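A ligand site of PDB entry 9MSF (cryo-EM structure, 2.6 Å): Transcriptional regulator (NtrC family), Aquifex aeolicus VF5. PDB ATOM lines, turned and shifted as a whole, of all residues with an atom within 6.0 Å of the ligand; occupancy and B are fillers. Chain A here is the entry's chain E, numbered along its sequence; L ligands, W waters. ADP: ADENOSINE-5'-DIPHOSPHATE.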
ATOM      1  N   GLU A  19       7.801  27.953 -15.074  1.00  0.00           N
ATOM      2  CA  GLU A  19       7.705  27.146 -13.859  1.00  0.00           C
ATOM      3  C   GLU A  19       6.636  26.067 -13.984  1.00  0.00           C
ATOM      4  O   GLU A  19       5.517  26.326 -14.432  1.00  0.00           O
ATOM      5  CB  GLU A  19       7.409  28.041 -12.657  1.00  0.00           C
ATOM      6  CG  GLU A  19       8.584  28.900 -12.216  1.00  0.00           C
ATOM      7  CD  GLU A  19       9.705  28.078 -11.593  1.00  0.00           C
ATOM      8  OE1 GLU A  19       9.441  26.948 -11.155  1.00  0.00           O
ATOM      9  OE2 GLU A  19      10.854  28.581 -11.550  1.00  0.00           O
ATOM     10  N   TYR A  20       6.988  24.850 -13.573  1.00  0.00           N
ATOM     11  CA  TYR A  20       6.095  23.708 -13.632  1.00  0.00           C
ATOM     12  C   TYR A  20       6.034  23.052 -12.264  1.00  0.00           C
ATOM     13  O   TYR A  20       6.963  23.169 -11.457  1.00  0.00           O
ATOM     14  CB  TYR A  20       6.558  22.692 -14.687  1.00  0.00           C
ATOM     15  CG  TYR A  20       6.529  23.227 -16.094  1.00  0.00           C
ATOM     16  CD1 TYR A  20       5.439  23.942 -16.563  1.00  0.00           C
ATOM     17  CD2 TYR A  20       7.605  23.016 -16.960  1.00  0.00           C
ATOM     18  CE1 TYR A  20       5.412  24.429 -17.861  1.00  0.00           C
ATOM     19  CE2 TYR A  20       7.579  23.502 -18.245  1.00  0.00           C
ATOM     20  CZ  TYR A  20       6.482  24.213 -18.698  1.00  0.00           C
ATOM     21  OH  TYR A  20       6.466  24.701 -19.984  1.00  0.00           O
ATOM     22  N   VAL A  21       4.931  22.355 -12.002  1.00  0.00           N
ATOM     23  CA  VAL A  21       4.665  21.748 -10.706  1.00  0.00           C
ATOM     24  C   VAL A  21       4.837  20.245 -10.828  1.00  0.00           C
ATOM     25  O   VAL A  21       4.161  19.596 -11.642  1.00  0.00           O
ATOM     26  CB  VAL A  21       3.259  22.103 -10.199  1.00  0.00           C
ATOM     27  CG1 VAL A  21       3.038  21.527  -8.812  1.00  0.00           C
ATOM     28  CG2 VAL A  21       3.063  23.613 -10.196  1.00  0.00           C
ATOM     29  N   PHE A  22       5.733  19.689 -10.014  1.00  0.00           N
ATOM     30  CA  PHE A  22       5.949  18.233  -9.920  1.00  0.00           C
ATOM     31  C   PHE A  22       6.092  17.915  -8.441  1.00  0.00           C
ATOM     32  O   PHE A  22       7.185  17.961  -7.883  1.00  0.00           O
ATOM     33  CB  PHE A  22       7.186  17.802 -10.716  1.00  0.00           C
ATOM     34  CG  PHE A  22       7.115  18.132 -12.174  1.00  0.00           C
ATOM     35  CD1 PHE A  22       6.312  17.390 -13.026  1.00  0.00           C
ATOM     36  CD2 PHE A  22       7.852  19.171 -12.706  1.00  0.00           C
ATOM     37  CE1 PHE A  22       6.249  17.688 -14.375  1.00  0.00           C
ATOM     38  CE2 PHE A  22       7.799  19.478 -14.047  1.00  0.00           C
ATOM     39  CZ  PHE A  22       6.988  18.731 -14.885  1.00  0.00           C
ATOM     40  N   GLU A  49      -3.271  10.165 -20.727  1.00  0.00           N
ATOM     41  CA  GLU A  49      -4.596  10.635 -21.117  1.00  0.00           C
ATOM     42  C   GLU A  49      -4.455  12.017 -21.770  1.00  0.00           C
ATOM     43  O   GLU A  49      -3.344  12.479 -22.059  1.00  0.00           O
ATOM     44  CB  GLU A  49      -5.529  10.652 -19.916  1.00  0.00           C
ATOM     45  CG  GLU A  49      -5.782   9.274 -19.333  1.00  0.00           C
ATOM     46  CD  GLU A  49      -6.928   9.265 -18.336  1.00  0.00           C
ATOM     47  OE1 GLU A  49      -7.652  10.278 -18.247  1.00  0.00           O
ATOM     48  OE2 GLU A  49      -7.104   8.242 -17.637  1.00  0.00           O
ATOM     49  N   SER A  50      -5.573  12.700 -21.994  1.00  0.00           N
ATOM     50  CA  SER A  50      -5.566  13.994 -22.640  1.00  0.00           C
ATOM     51  C   SER A  50      -5.543  15.096 -21.584  1.00  0.00           C
ATOM     52  O   SER A  50      -6.404  15.138 -20.707  1.00  0.00           O
ATOM     53  CB  SER A  50      -6.787  14.161 -23.547  1.00  0.00           C
ATOM     54  OG  SER A  50      -6.739  15.386 -24.251  1.00  0.00           O
ATOM     55  N   GLY A  51      -4.546  15.978 -21.677  1.00  0.00           N
ATOM     56  CA  GLY A  51      -4.396  17.057 -20.722  1.00  0.00           C
ATOM     57  C   GLY A  51      -3.510  16.768 -19.547  1.00  0.00           C
ATOM     58  O   GLY A  51      -3.542  17.528 -18.566  1.00  0.00           O
ATOM     59  N   VAL A  52      -2.708  15.707 -19.596  1.00  0.00           N
ATOM     60  CA  VAL A  52      -1.886  15.322 -18.454  1.00  0.00           C
ATOM     61  C   VAL A  52      -0.508  15.975 -18.459  1.00  0.00           C
ATOM     62  O   VAL A  52       0.139  16.051 -17.401  1.00  0.00           O
ATOM     63  CB  VAL A  52      -1.739  13.801 -18.365  1.00  0.00           C
ATOM     64  CG1 VAL A  52      -3.074  13.158 -18.055  1.00  0.00           C
ATOM     65  CG2 VAL A  52      -1.180  13.248 -19.666  1.00  0.00           C
ATOM     66  N   GLY A  53      -0.028  16.434 -19.610  1.00  0.00           N
ATOM     67  CA  GLY A  53       1.259  17.104 -19.657  1.00  0.00           C
ATOM     68  C   GLY A  53       2.305  16.434 -20.524  1.00  0.00           C
ATOM     69  O   GLY A  53       3.503  16.530 -20.219  1.00  0.00           O
ATOM     70  N   LYS A  54       1.889  15.747 -21.582  1.00  0.00           N
ATOM     71  CA  LYS A  54       2.840  15.080 -22.456  1.00  0.00           C
ATOM     72  C   LYS A  54       3.776  16.083 -23.137  1.00  0.00           C
ATOM     73  O   LYS A  54       4.995  15.857 -23.203  1.00  0.00           O
ATOM     74  CB  LYS A  54       2.110  14.239 -23.506  1.00  0.00           C
ATOM     75  CG  LYS A  54       1.429  13.010 -22.943  1.00  0.00           C
ATOM     76  CD  LYS A  54       0.793  12.183 -24.047  1.00  0.00           C
ATOM     77  CE  LYS A  54      -0.434  12.862 -24.609  1.00  0.00           C
ATOM     78  NZ  LYS A  54      -1.517  12.958 -23.585  1.00  0.00           N
ATOM     79  N   GLU A  55       3.224  17.179 -23.644  1.00  0.00           N
ATOM     80  CA  GLU A  55       4.071  18.164 -24.328  1.00  0.00           C
ATOM     81  C   GLU A  55       4.971  18.904 -23.346  1.00  0.00           C
ATOM     82  O   GLU A  55       6.094  19.284 -23.698  1.00  0.00           O
ATOM     83  CB  GLU A  55       3.194  19.150 -25.107  1.00  0.00           C
ATOM     84  CG  GLU A  55       3.986  20.086 -26.007  1.00  0.00           C
ATOM     85  CD  GLU A  55       3.092  20.906 -26.914  1.00  0.00           C
ATOM     86  OE1 GLU A  55       1.880  20.628 -26.975  1.00  0.00           O
ATOM     87  OE2 GLU A  55       3.603  21.844 -27.558  1.00  0.00           O
ATOM     88  N   VAL A  56       4.505  19.107 -22.106  1.00  0.00           N
ATOM     89  CA  VAL A  56       5.362  19.694 -21.088  1.00  0.00           C
ATOM     90  C   VAL A  56       6.573  18.797 -20.827  1.00  0.00           C
ATOM     91  O   VAL A  56       7.702  19.280 -20.734  1.00  0.00           O
ATOM     92  CB  VAL A  56       4.561  19.949 -19.794  1.00  0.00           C
ATOM     93  CG1 VAL A  56       5.467  20.445 -18.694  1.00  0.00           C
ATOM     94  CG2 VAL A  56       3.442  20.938 -20.055  1.00  0.00           C
ATOM     95  N   VAL A  57       6.343  17.495 -20.720  1.00  0.00           N
ATOM     96  CA  VAL A  57       7.435  16.559 -20.498  1.00  0.00           C
ATOM     97  C   VAL A  57       8.360  16.528 -21.714  1.00  0.00           C
ATOM     98  O   VAL A  57       9.585  16.422 -21.571  1.00  0.00           O
ATOM     99  CB  VAL A  57       6.891  15.161 -20.165  1.00  0.00           C
ATOM    100  CG1 VAL A  57       8.013  14.148 -20.109  1.00  0.00           C
ATOM    101  CG2 VAL A  57       6.143  15.196 -18.844  1.00  0.00           C
ATOM    102  N   ASP A 119       2.956  14.924 -32.259  1.00  0.00           N
ATOM    103  CA  ASP A 119       1.812  14.859 -31.357  1.00  0.00           C
ATOM    104  C   ASP A 119       0.690  14.042 -31.987  1.00  0.00           C
ATOM    105  O   ASP A 119       0.415  14.163 -33.192  1.00  0.00           O
ATOM    106  CB  ASP A 119       1.315  16.265 -31.022  1.00  0.00           C
ATOM    107  CG  ASP A 119       0.403  16.285 -29.809  1.00  0.00           C
ATOM    108  OD1 ASP A 119       0.250  15.224 -29.168  1.00  0.00           O
ATOM    109  OD2 ASP A 119      -0.156  17.355 -29.505  1.00  0.00           O
ATOM    110  N   ARG A 194      -3.322  11.752  -9.189  1.00  0.00           N
ATOM    111  CA  ARG A 194      -2.344  12.651  -8.578  1.00  0.00           C
ATOM    112  C   ARG A 194      -3.105  13.564  -7.625  1.00  0.00           C
ATOM    113  O   ARG A 194      -3.480  14.681  -7.988  1.00  0.00           O
ATOM    114  CB  ARG A 194      -1.581  13.449  -9.651  1.00  0.00           C
ATOM    115  CG  ARG A 194      -0.829  12.600 -10.651  1.00  0.00           C
ATOM    116  CD  ARG A 194      -0.752  13.281 -12.011  1.00  0.00           C
ATOM    117  NE  ARG A 194      -0.034  14.544 -11.976  1.00  0.00           N
ATOM    118  CZ  ARG A 194       0.136  15.331 -13.024  1.00  0.00           C
ATOM    119  NH1 ARG A 194      -0.346  15.012 -14.217  1.00  0.00           N
ATOM    120  NH2 ARG A 194       0.823  16.468 -12.887  1.00  0.00           N
ATOM    121  N   ASP A 197      -0.978  16.613  -6.313  1.00  0.00           N
ATOM    122  CA  ASP A 197      -0.583  17.548  -7.358  1.00  0.00           C
ATOM    123  C   ASP A 197      -1.766  18.371  -7.886  1.00  0.00           C
ATOM    124  O   ASP A 197      -1.747  18.815  -9.039  1.00  0.00           O
ATOM    125  CB  ASP A 197       0.098  16.798  -8.509  1.00  0.00           C
ATOM    126  CG  ASP A 197       1.015  17.686  -9.317  1.00  0.00           C
ATOM    127  OD1 ASP A 197       1.132  18.878  -8.991  1.00  0.00           O
ATOM    128  OD2 ASP A 197       1.630  17.183 -10.280  1.00  0.00           O
ATOM    129  N   LEU A 201      -1.115  23.106  -8.355  1.00  0.00           N
ATOM    130  CA  LEU A 201      -1.473  23.527  -9.709  1.00  0.00           C
ATOM    131  C   LEU A 201      -2.599  24.547  -9.685  1.00  0.00           C
ATOM    132  O   LEU A 201      -2.584  25.520 -10.455  1.00  0.00           O
ATOM    133  CB  LEU A 201      -1.868  22.310 -10.540  1.00  0.00           C
ATOM    134  CG  LEU A 201      -0.731  21.492 -11.159  1.00  0.00           C
ATOM    135  CD1 LEU A 201      -1.279  20.278 -11.889  1.00  0.00           C
ATOM    136  CD2 LEU A 201       0.084  22.358 -12.093  1.00  0.00           C
ATOM    137  N   HIS A 204      -1.106  27.847  -8.653  1.00  0.00           N
ATOM    138  CA  HIS A 204      -0.325  28.417  -9.745  1.00  0.00           C
ATOM    139  C   HIS A 204      -1.234  29.047 -10.798  1.00  0.00           C
ATOM    140  O   HIS A 204      -1.001  30.172 -11.247  1.00  0.00           O
ATOM    141  CB  HIS A 204       0.552  27.335 -10.370  1.00  0.00           C
ATOM    142  CG  HIS A 204       1.347  27.800 -11.558  1.00  0.00           C
ATOM    143  ND1 HIS A 204       1.710  26.963 -12.588  1.00  0.00           N
ATOM    144  CD2 HIS A 204       1.851  29.018 -11.873  1.00  0.00           C
ATOM    145  CE1 HIS A 204       2.397  27.641 -13.479  1.00  0.00           C
ATOM    146  NE2 HIS A 204       2.500  28.890 -13.071  1.00  0.00           N
ATOM    147  N   PHE A 205      -2.299  28.327 -11.185  1.00  0.00           N
ATOM    148  CA  PHE A 205      -3.233  28.874 -12.168  1.00  0.00           C
ATOM    149  C   PHE A 205      -3.955  30.097 -11.625  1.00  0.00           C
ATOM    150  O   PHE A 205      -4.192  31.061 -12.353  1.00  0.00           O
ATOM    151  CB  PHE A 205      -4.231  27.792 -12.585  1.00  0.00           C
ATOM    152  CG  PHE A 205      -3.625  26.711 -13.424  1.00  0.00           C
ATOM    153  CD1 PHE A 205      -2.469  26.945 -14.139  1.00  0.00           C
ATOM    154  CD2 PHE A 205      -4.217  25.458 -13.496  1.00  0.00           C
ATOM    155  CE1 PHE A 205      -1.906  25.947 -14.917  1.00  0.00           C
ATOM    156  CE2 PHE A 205      -3.665  24.464 -14.265  1.00  0.00           C
ATOM    157  CZ  PHE A 205      -2.501  24.715 -14.980  1.00  0.00           C
ATOM    158  N   VAL A 237      -5.263  18.565 -16.344  1.00  0.00           N
ATOM    159  CA  VAL A 237      -4.775  19.911 -16.085  1.00  0.00           C
ATOM    160  C   VAL A 237      -5.435  20.916 -17.014  1.00  0.00           C
ATOM    161  O   VAL A 237      -5.615  22.076 -16.643  1.00  0.00           O
ATOM    162  CB  VAL A 237      -3.239  19.944 -16.211  1.00  0.00           C
ATOM    163  CG1 VAL A 237      -2.698  21.284 -15.759  1.00  0.00           C
ATOM    164  CG2 VAL A 237      -2.625  18.810 -15.401  1.00  0.00           C
ATOM    165  N   ARG A 238      -5.823  20.493 -18.213  1.00  0.00           N
ATOM    166  CA  ARG A 238      -6.539  21.389 -19.128  1.00  0.00           C
ATOM    167  C   ARG A 238      -7.852  21.841 -18.513  1.00  0.00           C
ATOM    168  O   ARG A 238      -8.152  23.052 -18.471  1.00  0.00           O
ATOM    169  CB  ARG A 238      -6.775  20.683 -20.460  1.00  0.00           C
ATOM    170  CG  ARG A 238      -7.436  21.541 -21.517  1.00  0.00           C
ATOM    171  CD  ARG A 238      -6.399  22.318 -22.300  1.00  0.00           C
ATOM    172  NE  ARG A 238      -5.306  21.456 -22.753  1.00  0.00           N
ATOM    173  CZ  ARG A 238      -5.374  20.651 -23.804  1.00  0.00           C
ATOM    174  NH1 ARG A 238      -6.477  20.559 -24.540  1.00  0.00           N
ATOM    175  NH2 ARG A 238      -4.316  19.915 -24.127  1.00  0.00           N
ATOM    176  N   LYS A 241      -7.253  24.129 -15.504  1.00  0.00           N
ATOM    177  CA  LYS A 241      -6.882  25.481 -15.912  1.00  0.00           C
ATOM    178  C   LYS A 241      -8.101  26.254 -16.405  1.00  0.00           C
ATOM    179  O   LYS A 241      -8.268  27.429 -16.070  1.00  0.00           O
ATOM    180  CB  LYS A 241      -5.808  25.402 -16.997  1.00  0.00           C
ATOM    181  CG  LYS A 241      -5.058  26.704 -17.250  1.00  0.00           C
ATOM    182  CD  LYS A 241      -3.933  26.482 -18.254  1.00  0.00           C
ATOM    183  CE  LYS A 241      -3.076  27.713 -18.424  1.00  0.00           C
ATOM    184  NZ  LYS A 241      -1.951  27.480 -19.357  1.00  0.00           N
HETATM  185  PB  ADP L   1      -1.413  17.443 -23.542  1.00  0.00           P
HETATM  186  O1B ADP L   1      -2.920  17.379 -23.503  1.00  0.00           O
HETATM  187  O2B ADP L   1      -0.807  16.885 -24.800  1.00  0.00           O
HETATM  188  O3B ADP L   1      -0.778  16.946 -22.266  1.00  0.00           O
HETATM  189  PA  ADP L   1       0.028  19.772 -22.722  1.00  0.00           P
HETATM  190  O1A ADP L   1       0.393  21.043 -23.443  1.00  0.00           O
HETATM  191  O2A ADP L   1       1.112  18.792 -22.382  1.00  0.00           O
HETATM  192  O3A ADP L   1      -1.087  19.022 -23.611  1.00  0.00           O
HETATM  193  O5' ADP L   1      -0.715  20.211 -21.361  1.00  0.00           O
HETATM  194  C5' ADP L   1      -1.950  20.923 -21.377  1.00  0.00           C
HETATM  195  C4' ADP L   1      -1.805  22.163 -20.514  1.00  0.00           C
HETATM  196  O4' ADP L   1      -1.653  21.804 -19.129  1.00  0.00           O
HETATM  197  C3' ADP L   1      -0.564  22.962 -20.905  1.00  0.00           C
HETATM  198  O3' ADP L   1      -0.941  24.241 -21.413  1.00  0.00           O
HETATM  199  C2' ADP L   1       0.250  23.126 -19.643  1.00  0.00           C
HETATM  200  O2' ADP L   1       0.539  24.511 -19.423  1.00  0.00           O
HETATM  201  C1' ADP L   1      -0.616  22.577 -18.522  1.00  0.00           C
HETATM  202  N9  ADP L   1       0.183  21.723 -17.620  1.00  0.00           N
HETATM  203  C8  ADP L   1       0.216  20.374 -17.651  1.00  0.00           C
HETATM  204  N7  ADP L   1       1.040  19.889 -16.695  1.00  0.00           N
HETATM  205  C5  ADP L   1       1.559  20.932 -16.028  1.00  0.00           C
HETATM  206  C6  ADP L   1       2.499  21.115 -14.896  1.00  0.00           C
HETATM  207  N6  ADP L   1       3.065  20.049 -14.286  1.00  0.00           N
HETATM  208  N1  ADP L   1       2.772  22.374 -14.511  1.00  0.00           N
HETATM  209  C2  ADP L   1       2.215  23.443 -15.122  1.00  0.00           C
HETATM  210  N3  ADP L   1       1.350  23.346 -16.151  1.00  0.00           N
HETATM  211  C4  ADP L   1       0.991  22.138 -16.640  1.00  0.00           C
HETATM  212  O   HOH W   1      -1.048  18.068 -27.076  1.00  0.00           O
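The backbone NH (N) of Glu 55 lies within hydrogen-bond range of an oxygen (O2A) of the ligand (2.9 Å).
An oxygen (O3B) of the ligand is in hydrogen-bond range of the backbone NH (N) of Gly 53 (2.8 Å).
O of Val 21 is in hydrogen-bond range of N6 of the ligand, at 2.9 Å.
The backbone NH of Val 21 sits at hydrogen-bond distance from a nitrogen (N1) of the ligand (3.3 Å).
The guanidinium group (NH2) of Arg 238 is in salt-bridge range of an oxygen (O1B) of the ligand, at 3.0 Å.
O1B of the ligand lies within hydrogen-bond range of N of Gly 51, 2.8 Å away.
An oxygen (O3B) of the ligand is in hydrogen-bond range of the backbone NH (N) of Lys 54, at 3.0 Å.
N of Val 56 is in hydrogen-bond range of O2A of the ligand (3.4 Å).
The side-chain amino group of Lys 54 sits at hydrogen-bond distance from the backbone carbonyl oxygen of Glu 49.
The backbone NH (N) of Val 237 is in hydrogen-bond range of the backbone carbonyl oxygen (O) of Gly 51 (3.0 Å).
The backbone carbonyl oxygen of Val 52 sits at hydrogen-bond distance from the guanidinium group of Arg 194 (3.4 Å).
Water W1 lies within hydrogen-bond range of an oxygen (O2B) of the ligand (2.6 Å) and the side-chain carboxylate (OD2) of Asp 119 (2.7 Å).
Tyr 20 touches the ligand (CD1 to C2, 3.6 Å).
Phe 22 touches the ligand.
Ser 50 touches the ligand.
N of Val 52 touches O3B of the ligand, at 3.5 Å.
Leu 201 touches the ligand.
Val 237 touches the ligand (CG1 to N9, 3.5 Å).
Lys 241 touches the ligand.
Within 4 Å of the ligand: Tyr 20, Val 21, Phe 22, Ser 50, Gly 51, Val 52, Gly 53, Lys 54, Glu 55, Val 56, Leu 201, Val 237, Arg 238 and Lys 241.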
